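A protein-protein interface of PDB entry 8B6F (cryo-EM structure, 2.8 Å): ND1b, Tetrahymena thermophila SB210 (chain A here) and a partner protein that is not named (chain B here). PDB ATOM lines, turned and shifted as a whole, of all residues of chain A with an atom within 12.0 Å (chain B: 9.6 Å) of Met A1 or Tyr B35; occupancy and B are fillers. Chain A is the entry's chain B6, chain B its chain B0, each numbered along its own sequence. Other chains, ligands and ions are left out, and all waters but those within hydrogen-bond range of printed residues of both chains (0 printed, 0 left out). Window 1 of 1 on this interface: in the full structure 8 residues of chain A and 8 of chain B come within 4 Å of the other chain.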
ATOM      1  N   MET A   1      -1.819 -10.244  24.301  1.00  0.00           N
ATOM      2  CA  MET A   1      -2.728  -9.542  25.249  1.00  0.00           C
ATOM      3  C   MET A   1      -4.078 -10.242  25.326  1.00  0.00           C
ATOM      4  O   MET A   1      -4.471 -10.945  24.395  1.00  0.00           O
ATOM      5  CB  MET A   1      -2.917  -8.083  24.829  1.00  0.00           C
ATOM      6  CG  MET A   1      -1.759  -7.181  25.212  1.00  0.00           C
ATOM      7  SD  MET A   1      -1.595  -6.981  26.995  1.00  0.00           S
ATOM      8  CE  MET A   1      -0.115  -5.981  27.087  1.00  0.00           C
ATOM      9  N   PRO A   2      -4.791 -10.050  26.436  1.00  0.00           N
ATOM     10  CA  PRO A   2      -6.074 -10.750  26.604  1.00  0.00           C
ATOM     11  C   PRO A   2      -7.089 -10.442  25.521  1.00  0.00           C
ATOM     12  O   PRO A   2      -7.885 -11.322  25.170  1.00  0.00           O
ATOM     13  CB  PRO A   2      -6.555 -10.271  27.983  1.00  0.00           C
ATOM     14  CG  PRO A   2      -5.790  -9.030  28.259  1.00  0.00           C
ATOM     15  CD  PRO A   2      -4.468  -9.208  27.600  1.00  0.00           C
ATOM     16  N   TYR A   3      -7.097  -9.226  24.976  1.00  0.00           N
ATOM     17  CA  TYR A   3      -8.127  -8.870  24.008  1.00  0.00           C
ATOM     18  C   TYR A   3      -7.999  -9.656  22.710  1.00  0.00           C
ATOM     19  O   TYR A   3      -8.985  -9.780  21.980  1.00  0.00           O
ATOM     20  CB  TYR A   3      -8.105  -7.364  23.731  1.00  0.00           C
ATOM     21  CG  TYR A   3      -6.779  -6.802  23.281  1.00  0.00           C
ATOM     22  CD1 TYR A   3      -6.350  -6.941  21.970  1.00  0.00           C
ATOM     23  CD2 TYR A   3      -5.972  -6.097  24.162  1.00  0.00           C
ATOM     24  CE1 TYR A   3      -5.146  -6.414  21.554  1.00  0.00           C
ATOM     25  CE2 TYR A   3      -4.766  -5.566  23.757  1.00  0.00           C
ATOM     26  CZ  TYR A   3      -4.358  -5.728  22.451  1.00  0.00           C
ATOM     27  OH  TYR A   3      -3.158  -5.200  22.039  1.00  0.00           O
ATOM     28  N   PHE A   4      -6.830 -10.230  22.425  1.00  0.00           N
ATOM     29  CA  PHE A   4      -6.705 -11.095  21.257  1.00  0.00           C
ATOM     30  C   PHE A   4      -7.605 -12.317  21.392  1.00  0.00           C
ATOM     31  O   PHE A   4      -8.403 -12.617  20.497  1.00  0.00           O
ATOM     32  CB  PHE A   4      -5.244 -11.511  21.074  1.00  0.00           C
ATOM     33  CG  PHE A   4      -4.951 -12.137  19.741  1.00  0.00           C
ATOM     34  CD1 PHE A   4      -5.088 -11.409  18.573  1.00  0.00           C
ATOM     35  CD2 PHE A   4      -4.504 -13.445  19.659  1.00  0.00           C
ATOM     36  CE1 PHE A   4      -4.809 -11.977  17.346  1.00  0.00           C
ATOM     37  CE2 PHE A   4      -4.222 -14.019  18.434  1.00  0.00           C
ATOM     38  CZ  PHE A   4      -4.375 -13.283  17.276  1.00  0.00           C
ATOM     39  N   VAL A   5      -7.490 -13.037  22.507  1.00  0.00           N
ATOM     40  CA  VAL A   5      -8.351 -14.192  22.733  1.00  0.00           C
ATOM     41  C   VAL A   5      -9.806 -13.758  22.873  1.00  0.00           C
ATOM     42  O   VAL A   5     -10.720 -14.453  22.419  1.00  0.00           O
ATOM     43  CB  VAL A   5      -7.875 -14.975  23.968  1.00  0.00           C
ATOM     44  CG1 VAL A   5      -8.766 -16.183  24.210  1.00  0.00           C
ATOM     45  CG2 VAL A   5      -6.430 -15.405  23.796  1.00  0.00           C
ATOM     46  N   LEU A   6     -10.045 -12.608  23.506  1.00  0.00           N
ATOM     47  CA  LEU A   6     -11.413 -12.121  23.658  1.00  0.00           C
ATOM     48  C   LEU A   6     -12.048 -11.841  22.302  1.00  0.00           C
ATOM     49  O   LEU A   6     -13.216 -12.176  22.075  1.00  0.00           O
ATOM     50  CB  LEU A   6     -11.438 -10.871  24.538  1.00  0.00           C
ATOM     51  CG  LEU A   6     -12.823 -10.319  24.894  1.00  0.00           C
ATOM     52  CD1 LEU A   6     -13.707 -11.381  25.537  1.00  0.00           C
ATOM     53  CD2 LEU A   6     -12.693  -9.118  25.812  1.00  0.00           C
ATOM     54  N   LEU A   7     -11.293 -11.237  21.382  1.00  0.00           N
ATOM     55  CA  LEU A   7     -11.816 -11.000  20.041  1.00  0.00           C
ATOM     56  C   LEU A   7     -12.081 -12.311  19.312  1.00  0.00           C
ATOM     57  O   LEU A   7     -13.075 -12.433  18.589  1.00  0.00           O
ATOM     58  CB  LEU A   7     -10.853 -10.121  19.238  1.00  0.00           C
ATOM     59  CG  LEU A   7     -11.070  -8.600  19.259  1.00  0.00           C
ATOM     60  CD1 LEU A   7     -12.407  -8.235  18.641  1.00  0.00           C
ATOM     61  CD2 LEU A   7     -10.975  -8.011  20.653  1.00  0.00           C
ATOM     62  N   PHE A   8     -11.203 -13.300  19.480  1.00  0.00           N
ATOM     63  CA  PHE A   8     -11.458 -14.612  18.892  1.00  0.00           C
ATOM     64  C   PHE A   8     -12.789 -15.175  19.375  1.00  0.00           C
ATOM     65  O   PHE A   8     -13.601 -15.651  18.575  1.00  0.00           O
ATOM     66  CB  PHE A   8     -10.319 -15.571  19.237  1.00  0.00           C
ATOM     67  CG  PHE A   8      -9.346 -15.777  18.117  1.00  0.00           C
ATOM     68  CD1 PHE A   8      -9.607 -16.699  17.118  1.00  0.00           C
ATOM     69  CD2 PHE A   8      -8.165 -15.057  18.067  1.00  0.00           C
ATOM     70  CE1 PHE A   8      -8.712 -16.892  16.085  1.00  0.00           C
ATOM     71  CE2 PHE A   8      -7.264 -15.245  17.038  1.00  0.00           C
ATOM     72  CZ  PHE A   8      -7.537 -16.164  16.045  1.00  0.00           C
ATOM     73  N   LYS A   9     -13.030 -15.132  20.686  1.00  0.00           N
ATOM     74  CA  LYS A   9     -14.275 -15.670  21.223  1.00  0.00           C
ATOM     75  C   LYS A   9     -15.480 -14.873  20.738  1.00  0.00           C
ATOM     76  O   LYS A   9     -16.527 -15.450  20.431  1.00  0.00           O
ATOM     77  CB  LYS A   9     -14.224 -15.693  22.749  1.00  0.00           C
ATOM     78  CG  LYS A   9     -13.137 -16.593  23.304  1.00  0.00           C
ATOM     79  CD  LYS A   9     -13.332 -16.845  24.786  1.00  0.00           C
ATOM     80  CE  LYS A   9     -12.157 -17.613  25.364  1.00  0.00           C
ATOM     81  NZ  LYS A   9     -12.331 -17.898  26.810  1.00  0.00           N
ATOM     82  N   ILE A  10     -15.350 -13.548  20.655  1.00  0.00           N
ATOM     83  CA  ILE A  10     -16.453 -12.723  20.168  1.00  0.00           C
ATOM     84  C   ILE A  10     -16.787 -13.086  18.728  1.00  0.00           C
ATOM     85  O   ILE A  10     -17.961 -13.177  18.351  1.00  0.00           O
ATOM     86  CB  ILE A  10     -16.110 -11.230  20.305  1.00  0.00           C
ATOM     87  CG1 ILE A  10     -16.016 -10.837  21.777  1.00  0.00           C
ATOM     88  CG2 ILE A  10     -17.167 -10.373  19.621  1.00  0.00           C
ATOM     89  CD1 ILE A  10     -15.364  -9.496  22.000  1.00  0.00           C
ATOM     90  N   GLY B  27     -10.811  -4.884  15.175  1.00  0.00           N
ATOM     91  CA  GLY B  27     -10.925  -5.153  16.598  1.00  0.00           C
ATOM     92  C   GLY B  27      -9.624  -4.930  17.342  1.00  0.00           C
ATOM     93  O   GLY B  27      -9.619  -4.386  18.449  1.00  0.00           O
ATOM     94  N   LEU B  28      -8.505  -5.356  16.755  1.00  0.00           N
ATOM     95  CA  LEU B  28      -7.209  -5.078  17.362  1.00  0.00           C
ATOM     96  C   LEU B  28      -6.941  -3.581  17.418  1.00  0.00           C
ATOM     97  O   LEU B  28      -6.404  -3.076  18.412  1.00  0.00           O
ATOM     98  CB  LEU B  28      -6.102  -5.800  16.593  1.00  0.00           C
ATOM     99  CG  LEU B  28      -5.990  -7.306  16.847  1.00  0.00           C
ATOM    100  CD1 LEU B  28      -4.940  -7.920  15.943  1.00  0.00           C
ATOM    101  CD2 LEU B  28      -5.661  -7.595  18.304  1.00  0.00           C
ATOM    102  N   GLY B  29      -7.298  -2.854  16.359  1.00  0.00           N
ATOM    103  CA  GLY B  29      -7.152  -1.409  16.395  1.00  0.00           C
ATOM    104  C   GLY B  29      -7.939  -0.786  17.529  1.00  0.00           C
ATOM    105  O   GLY B  29      -7.427   0.052  18.274  1.00  0.00           O
ATOM    106  N   PHE B  30      -9.201  -1.190  17.677  1.00  0.00           N
ATOM    107  CA  PHE B  30     -10.044  -0.629  18.728  1.00  0.00           C
ATOM    108  C   PHE B  30      -9.488  -0.959  20.107  1.00  0.00           C
ATOM    109  O   PHE B  30      -9.403  -0.090  20.982  1.00  0.00           O
ATOM    110  CB  PHE B  30     -11.473  -1.152  18.578  1.00  0.00           C
ATOM    111  CG  PHE B  30     -12.422  -0.624  19.611  1.00  0.00           C
ATOM    112  CD1 PHE B  30     -13.012   0.617  19.456  1.00  0.00           C
ATOM    113  CD2 PHE B  30     -12.741  -1.377  20.727  1.00  0.00           C
ATOM    114  CE1 PHE B  30     -13.892   1.105  20.402  1.00  0.00           C
ATOM    115  CE2 PHE B  30     -13.622  -0.896  21.676  1.00  0.00           C
ATOM    116  CZ  PHE B  30     -14.198   0.347  21.513  1.00  0.00           C
ATOM    117  N   SER B  31      -9.115  -2.220  20.323  1.00  0.00           N
ATOM    118  CA  SER B  31      -8.599  -2.627  21.626  1.00  0.00           C
ATOM    119  C   SER B  31      -7.289  -1.918  21.949  1.00  0.00           C
ATOM    120  O   SER B  31      -7.075  -1.482  23.085  1.00  0.00           O
ATOM    121  CB  SER B  31      -8.408  -4.141  21.661  1.00  0.00           C
ATOM    122  OG  SER B  31      -9.639  -4.811  21.455  1.00  0.00           O
ATOM    123  N   THR B  32      -6.395  -1.808  20.966  1.00  0.00           N
ATOM    124  CA  THR B  32      -5.128  -1.120  21.198  1.00  0.00           C
ATOM    125  C   THR B  32      -5.341   0.362  21.470  1.00  0.00           C
ATOM    126  O   THR B  32      -4.641   0.951  22.301  1.00  0.00           O
ATOM    127  CB  THR B  32      -4.196  -1.324  20.005  1.00  0.00           C
ATOM    128  OG1 THR B  32      -3.883  -2.716  19.878  1.00  0.00           O
ATOM    129  CG2 THR B  32      -2.904  -0.533  20.174  1.00  0.00           C
ATOM    130  N   VAL B  33      -6.296   0.988  20.781  1.00  0.00           N
ATOM    131  CA  VAL B  33      -6.573   2.398  21.037  1.00  0.00           C
ATOM    132  C   VAL B  33      -7.066   2.585  22.466  1.00  0.00           C
ATOM    133  O   VAL B  33      -6.614   3.483  23.183  1.00  0.00           O
ATOM    134  CB  VAL B  33      -7.577   2.944  20.006  1.00  0.00           C
ATOM    135  CG1 VAL B  33      -8.193   4.259  20.472  1.00  0.00           C
ATOM    136  CG2 VAL B  33      -6.888   3.135  18.672  1.00  0.00           C
ATOM    137  N   ILE B  34      -7.988   1.730  22.909  1.00  0.00           N
ATOM    138  CA  ILE B  34      -8.472   1.831  24.283  1.00  0.00           C
ATOM    139  C   ILE B  34      -7.323   1.613  25.256  1.00  0.00           C
ATOM    140  O   ILE B  34      -7.172   2.350  26.237  1.00  0.00           O
ATOM    141  CB  ILE B  34      -9.623   0.838  24.527  1.00  0.00           C
ATOM    142  CG1 ILE B  34     -10.944   1.454  24.060  1.00  0.00           C
ATOM    143  CG2 ILE B  34      -9.696   0.433  26.005  1.00  0.00           C
ATOM    144  CD1 ILE B  34     -12.154   0.568  24.253  1.00  0.00           C
ATOM    145  N   TYR B  35      -6.499   0.597  25.003  1.00  0.00           N
ATOM    146  CA  TYR B  35      -5.392   0.293  25.902  1.00  0.00           C
ATOM    147  C   TYR B  35      -4.438   1.475  26.009  1.00  0.00           C
ATOM    148  O   TYR B  35      -4.013   1.849  27.106  1.00  0.00           O
ATOM    149  CB  TYR B  35      -4.660  -0.958  25.410  1.00  0.00           C
ATOM    150  CG  TYR B  35      -3.468  -1.362  26.248  1.00  0.00           C
ATOM    151  CD1 TYR B  35      -2.215  -0.803  26.027  1.00  0.00           C
ATOM    152  CD2 TYR B  35      -3.592  -2.314  27.248  1.00  0.00           C
ATOM    153  CE1 TYR B  35      -1.123  -1.176  26.788  1.00  0.00           C
ATOM    154  CE2 TYR B  35      -2.508  -2.693  28.012  1.00  0.00           C
ATOM    155  CZ  TYR B  35      -1.277  -2.120  27.777  1.00  0.00           C
ATOM    156  OH  TYR B  35      -0.194  -2.495  28.535  1.00  0.00           O
ATOM    157  N   ASP B  36      -4.088   2.076  24.871  1.00  0.00           N
ATOM    158  CA  ASP B  36      -3.159   3.201  24.887  1.00  0.00           C
ATOM    159  C   ASP B  36      -3.776   4.430  25.543  1.00  0.00           C
ATOM    160  O   ASP B  36      -3.098   5.147  26.285  1.00  0.00           O
ATOM    161  CB  ASP B  36      -2.709   3.522  23.464  1.00  0.00           C
ATOM    162  CG  ASP B  36      -2.013   2.358  22.801  1.00  0.00           C
ATOM    163  OD1 ASP B  36      -1.272   1.637  23.500  1.00  0.00           O
ATOM    164  OD2 ASP B  36      -2.205   2.163  21.587  1.00  0.00           O
ATOM    165  N   VAL B  37      -5.058   4.691  25.283  1.00  0.00           N
ATOM    166  CA  VAL B  37      -5.705   5.858  25.874  1.00  0.00           C
ATOM    167  C   VAL B  37      -5.724   5.746  27.392  1.00  0.00           C
ATOM    168  O   VAL B  37      -5.492   6.732  28.102  1.00  0.00           O
ATOM    169  CB  VAL B  37      -7.124   6.030  25.298  1.00  0.00           C
ATOM    170  CG1 VAL B  37      -7.902   7.090  26.068  1.00  0.00           C
ATOM    171  CG2 VAL B  37      -7.055   6.419  23.832  1.00  0.00           C
ATOM    172  N   VAL B  38      -6.007   4.553  27.917  1.00  0.00           N
ATOM    173  CA  VAL B  38      -6.032   4.363  29.366  1.00  0.00           C
ATOM    174  C   VAL B  38      -4.648   4.129  29.948  1.00  0.00           C
ATOM    175  O   VAL B  38      -4.482   4.207  31.170  1.00  0.00           O
ATOM    176  CB  VAL B  38      -6.947   3.186  29.754  1.00  0.00           C
ATOM    177  CG1 VAL B  38      -8.343   3.399  29.199  1.00  0.00           C
ATOM    178  CG2 VAL B  38      -6.368   1.855  29.280  1.00  0.00           C
ATOM    179  N   TYR B  39      -3.650   3.855  29.109  1.00  0.00           N
ATOM    180  CA  TYR B  39      -2.301   3.575  29.583  1.00  0.00           C
ATOM    181  C   TYR B  39      -1.443   4.829  29.664  1.00  0.00           C
ATOM    182  O   TYR B  39      -0.631   4.961  30.585  1.00  0.00           O
ATOM    183  CB  TYR B  39      -1.637   2.548  28.658  1.00  0.00           C
ATOM    184  CG  TYR B  39      -0.189   2.244  28.971  1.00  0.00           C
ATOM    185  CD1 TYR B  39       0.833   3.042  28.477  1.00  0.00           C
ATOM    186  CD2 TYR B  39       0.156   1.137  29.734  1.00  0.00           C
ATOM    187  CE1 TYR B  39       2.155   2.758  28.750  1.00  0.00           C
ATOM    188  CE2 TYR B  39       1.475   0.847  30.013  1.00  0.00           C
ATOM    189  CZ  TYR B  39       2.469   1.660  29.518  1.00  0.00           C
ATOM    190  OH  TYR B  39       3.783   1.371  29.793  1.00  0.00           O
ATOM    191  N   HIS B  40      -1.592   5.749  28.714  1.00  0.00           N
ATOM    192  CA  HIS B  40      -0.729   6.928  28.694  1.00  0.00           C
ATOM    193  C   HIS B  40      -0.875   7.781  29.945  1.00  0.00           C
ATOM    194  O   HIS B  40       0.154   8.129  30.551  1.00  0.00           O
ATOM    195  CB  HIS B  40      -1.012   7.749  27.434  1.00  0.00           C
ATOM    196  CG  HIS B  40      -0.095   8.918  27.261  1.00  0.00           C
ATOM    197  ND1 HIS B  40      -0.507  10.113  26.712  1.00  0.00           N
ATOM    198  CD2 HIS B  40       1.215   9.076  27.564  1.00  0.00           C
ATOM    199  CE1 HIS B  40       0.508  10.957  26.686  1.00  0.00           C
ATOM    200  NE2 HIS B  40       1.566  10.352  27.197  1.00  0.00           N
ATOM    201  N   PRO B  41      -2.079   8.158  30.383  1.00  0.00           N
ATOM    202  CA  PRO B  41      -2.170   9.054  31.550  1.00  0.00           C
ATOM    203  C   PRO B  41      -1.532   8.488  32.804  1.00  0.00           C
ATOM    204  O   PRO B  41      -0.914   9.236  33.571  1.00  0.00           O
ATOM    205  CB  PRO B  41      -3.684   9.248  31.722  1.00  0.00           C
ATOM    206  CG  PRO B  41      -4.281   8.870  30.418  1.00  0.00           C
ATOM    207  CD  PRO B  41      -3.410   7.789  29.877  1.00  0.00           C
ATOM    208  N   LYS B  42      -1.663   7.183  33.036  1.00  0.00           N
ATOM    209  CA  LYS B  42      -1.148   6.555  34.243  1.00  0.00           C
ATOM    210  C   LYS B  42       0.197   5.873  34.039  1.00  0.00           C
ATOM    211  O   LYS B  42       0.791   5.411  35.019  1.00  0.00           O
ATOM    212  CB  LYS B  42      -2.155   5.524  34.773  1.00  0.00           C
ATOM    213  CG  LYS B  42      -3.271   6.113  35.627  1.00  0.00           C
ATOM    214  CD  LYS B  42      -4.121   7.103  34.853  1.00  0.00           C
ATOM    215  CE  LYS B  42      -5.279   7.609  35.695  1.00  0.00           C
ATOM    216  NZ  LYS B  42      -6.095   8.617  34.965  1.00  0.00           N
ATOM    217  N   ASP B  43       0.687   5.793  32.806  1.00  0.00           N
ATOM    218  CA  ASP B  43       1.926   5.089  32.491  1.00  0.00           C
ATOM    219  C   ASP B  43       1.825   3.602  32.807  1.00  0.00           C
ATOM    220  O   ASP B  43       2.845   2.922  32.958  1.00  0.00           O
ATOM    221  CB  ASP B  43       3.112   5.711  33.235  1.00  0.00           C
ATOM    222  CG  ASP B  43       4.447   5.281  32.666  1.00  0.00           C
ATOM    223  OD1 ASP B  43       4.457   4.533  31.669  1.00  0.00           O
ATOM    224  OD2 ASP B  43       5.488   5.695  33.217  1.00  0.00           O
ATOM    225  N   ARG B  44       0.604   3.087  32.912  1.00  0.00           N
ATOM    226  CA  ARG B  44       0.353   1.693  33.251  1.00  0.00           C
ATOM    227  C   ARG B  44      -1.147   1.465  33.146  1.00  0.00           C
ATOM    228  O   ARG B  44      -1.925   2.405  32.961  1.00  0.00           O
ATOM    229  CB  ARG B  44       0.855   1.352  34.654  1.00  0.00           C
ATOM    230  CG  ARG B  44      -0.042   1.899  35.748  1.00  0.00           C
ATOM    231  CD  ARG B  44       0.648   1.928  37.094  1.00  0.00           C
ATOM    232  NE  ARG B  44      -0.218   2.508  38.111  1.00  0.00           N
ATOM    233  CZ  ARG B  44      -0.478   3.803  38.223  1.00  0.00           C
ATOM    234  NH1 ARG B  44       0.051   4.689  37.396  1.00  0.00           N
ATOM    235  NH2 ARG B  44      -1.290   4.220  39.191  1.00  0.00           N
ATOM    236  N   ILE B  45      -1.546   0.206  33.267  1.00  0.00           N
ATOM    237  CA  ILE B  45      -2.957  -0.167  33.354  1.00  0.00           C
ATOM    238  C   ILE B  45      -3.252  -0.319  34.841  1.00  0.00           C
ATOM    239  O   ILE B  45      -3.113  -1.398  35.419  1.00  0.00           O
ATOM    240  CB  ILE B  45      -3.267  -1.437  32.566  1.00  0.00           C
ATOM    241  CG1 ILE B  45      -2.890  -1.269  31.092  1.00  0.00           C
ATOM    242  CG2 ILE B  45      -4.742  -1.800  32.708  1.00  0.00           C
ATOM    243  CD1 ILE B  45      -3.661  -0.188  30.363  1.00  0.00           C
ATOM    244  N   GLU B  46      -3.664   0.777  35.472  1.00  0.00           N
ATOM    245  CA  GLU B  46      -3.946   0.746  36.899  1.00  0.00           C
ATOM    246  C   GLU B  46      -5.173  -0.110  37.175  1.00  0.00           C
ATOM    247  O   GLU B  46      -6.187  -0.017  36.480  1.00  0.00           O
ATOM    248  CB  GLU B  46      -4.163   2.160  37.438  1.00  0.00           C
ATOM    249  CG  GLU B  46      -5.362   2.883  36.846  1.00  0.00           C
ATOM    250  CD  GLU B  46      -5.666   4.179  37.568  1.00  0.00           C
ATOM    251  OE1 GLU B  46      -4.934   4.511  38.524  1.00  0.00           O
ATOM    252  OE2 GLU B  46      -6.636   4.864  37.184  1.00  0.00           O
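Among the printed residues, pairs that only touch across the chains: Met A1 with Tyr B35 (3.8 Å), Tyr A3 with Leu B28 (3.5 Å), Tyr A3 with Ser B31 (3.5 Å), Phe A4 with Leu B28 (3.9 Å), Leu A7 with Gly B27 (3.98 Å) and Leu A7 with Ser B31 (3.6 Å).
Of the 20 printed residues of chain B, 5 touch a printed residue of chain A. Printed residues of chain B that touch a printed residue of chain A: Gly B27, Leu B28, Ser B31, Thr B32 and Tyr B35. Hydrophobic or aromatic side chains of chain B that line the printed part of chain A: Leu B28 and Tyr B35. Printed residues of chain A that touch a printed residue of chain B: Met A1, Tyr A3, Phe A4 and Leu A7. Hydrophobic or aromatic side chains of chain A that line the printed part of chain B: Met A1, Tyr A3, Phe A4 and Leu A7. Among the printed residues, 7 pairs touch across the chains.
Met A1 touches just one residue of chain B: Tyr B35. Tyr B35 touches just one residue of chain A: Met A1 (3.8 Å). No residue of chain B comes within 4 Å of Pro A2. Ser B31 touches two residues of chain A. Of chain A, only Tyr A3 (3.4 Å) comes within 4 Å of Thr B32. No residue of chain A comes within 4 Å of Val B33. No residue of chain A comes within 4 Å of Asp B36. No residue of chain A comes within 4 Å of Ile B45. Printed residues of chain B within 4 Å of Phe A4: Leu B28 (3.9 Å). Of the printed residues of chain A, Gly B27 touches Leu A7 (3.98 Å). Of the printed residues of chain A, Leu B28 touches Tyr A3 and Phe A4. Printed residues of chain B within 4 Å of Leu A7: Gly B27 and Ser B31. The nearest residue of chain B that does not touch Met A1 is Ile B45 (6.8 Å). The nearest residue of chain A that does not touch Tyr B35 is Tyr A3 (4.9 Å). The nearest printed residue of chain B that does not touch Phe A4 is Ser B31 (6.2 Å).
The side-chain hydroxyl (OH) of Tyr A3 lies within hydrogen-bond range of the side-chain hydroxyl (OG1) of Thr B32, 3.4 Å away.
The backbone carbonyl oxygen of Gly B27 sits at hydrogen-bond distance from the side-chain hydroxyl of Ser B31, 3.0 Å away. The side-chain hydroxyl (OG1) of Thr B32 lies within hydrogen-bond range of the backbone carbonyl oxygen (O) of Leu B28 (2.9 Å).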
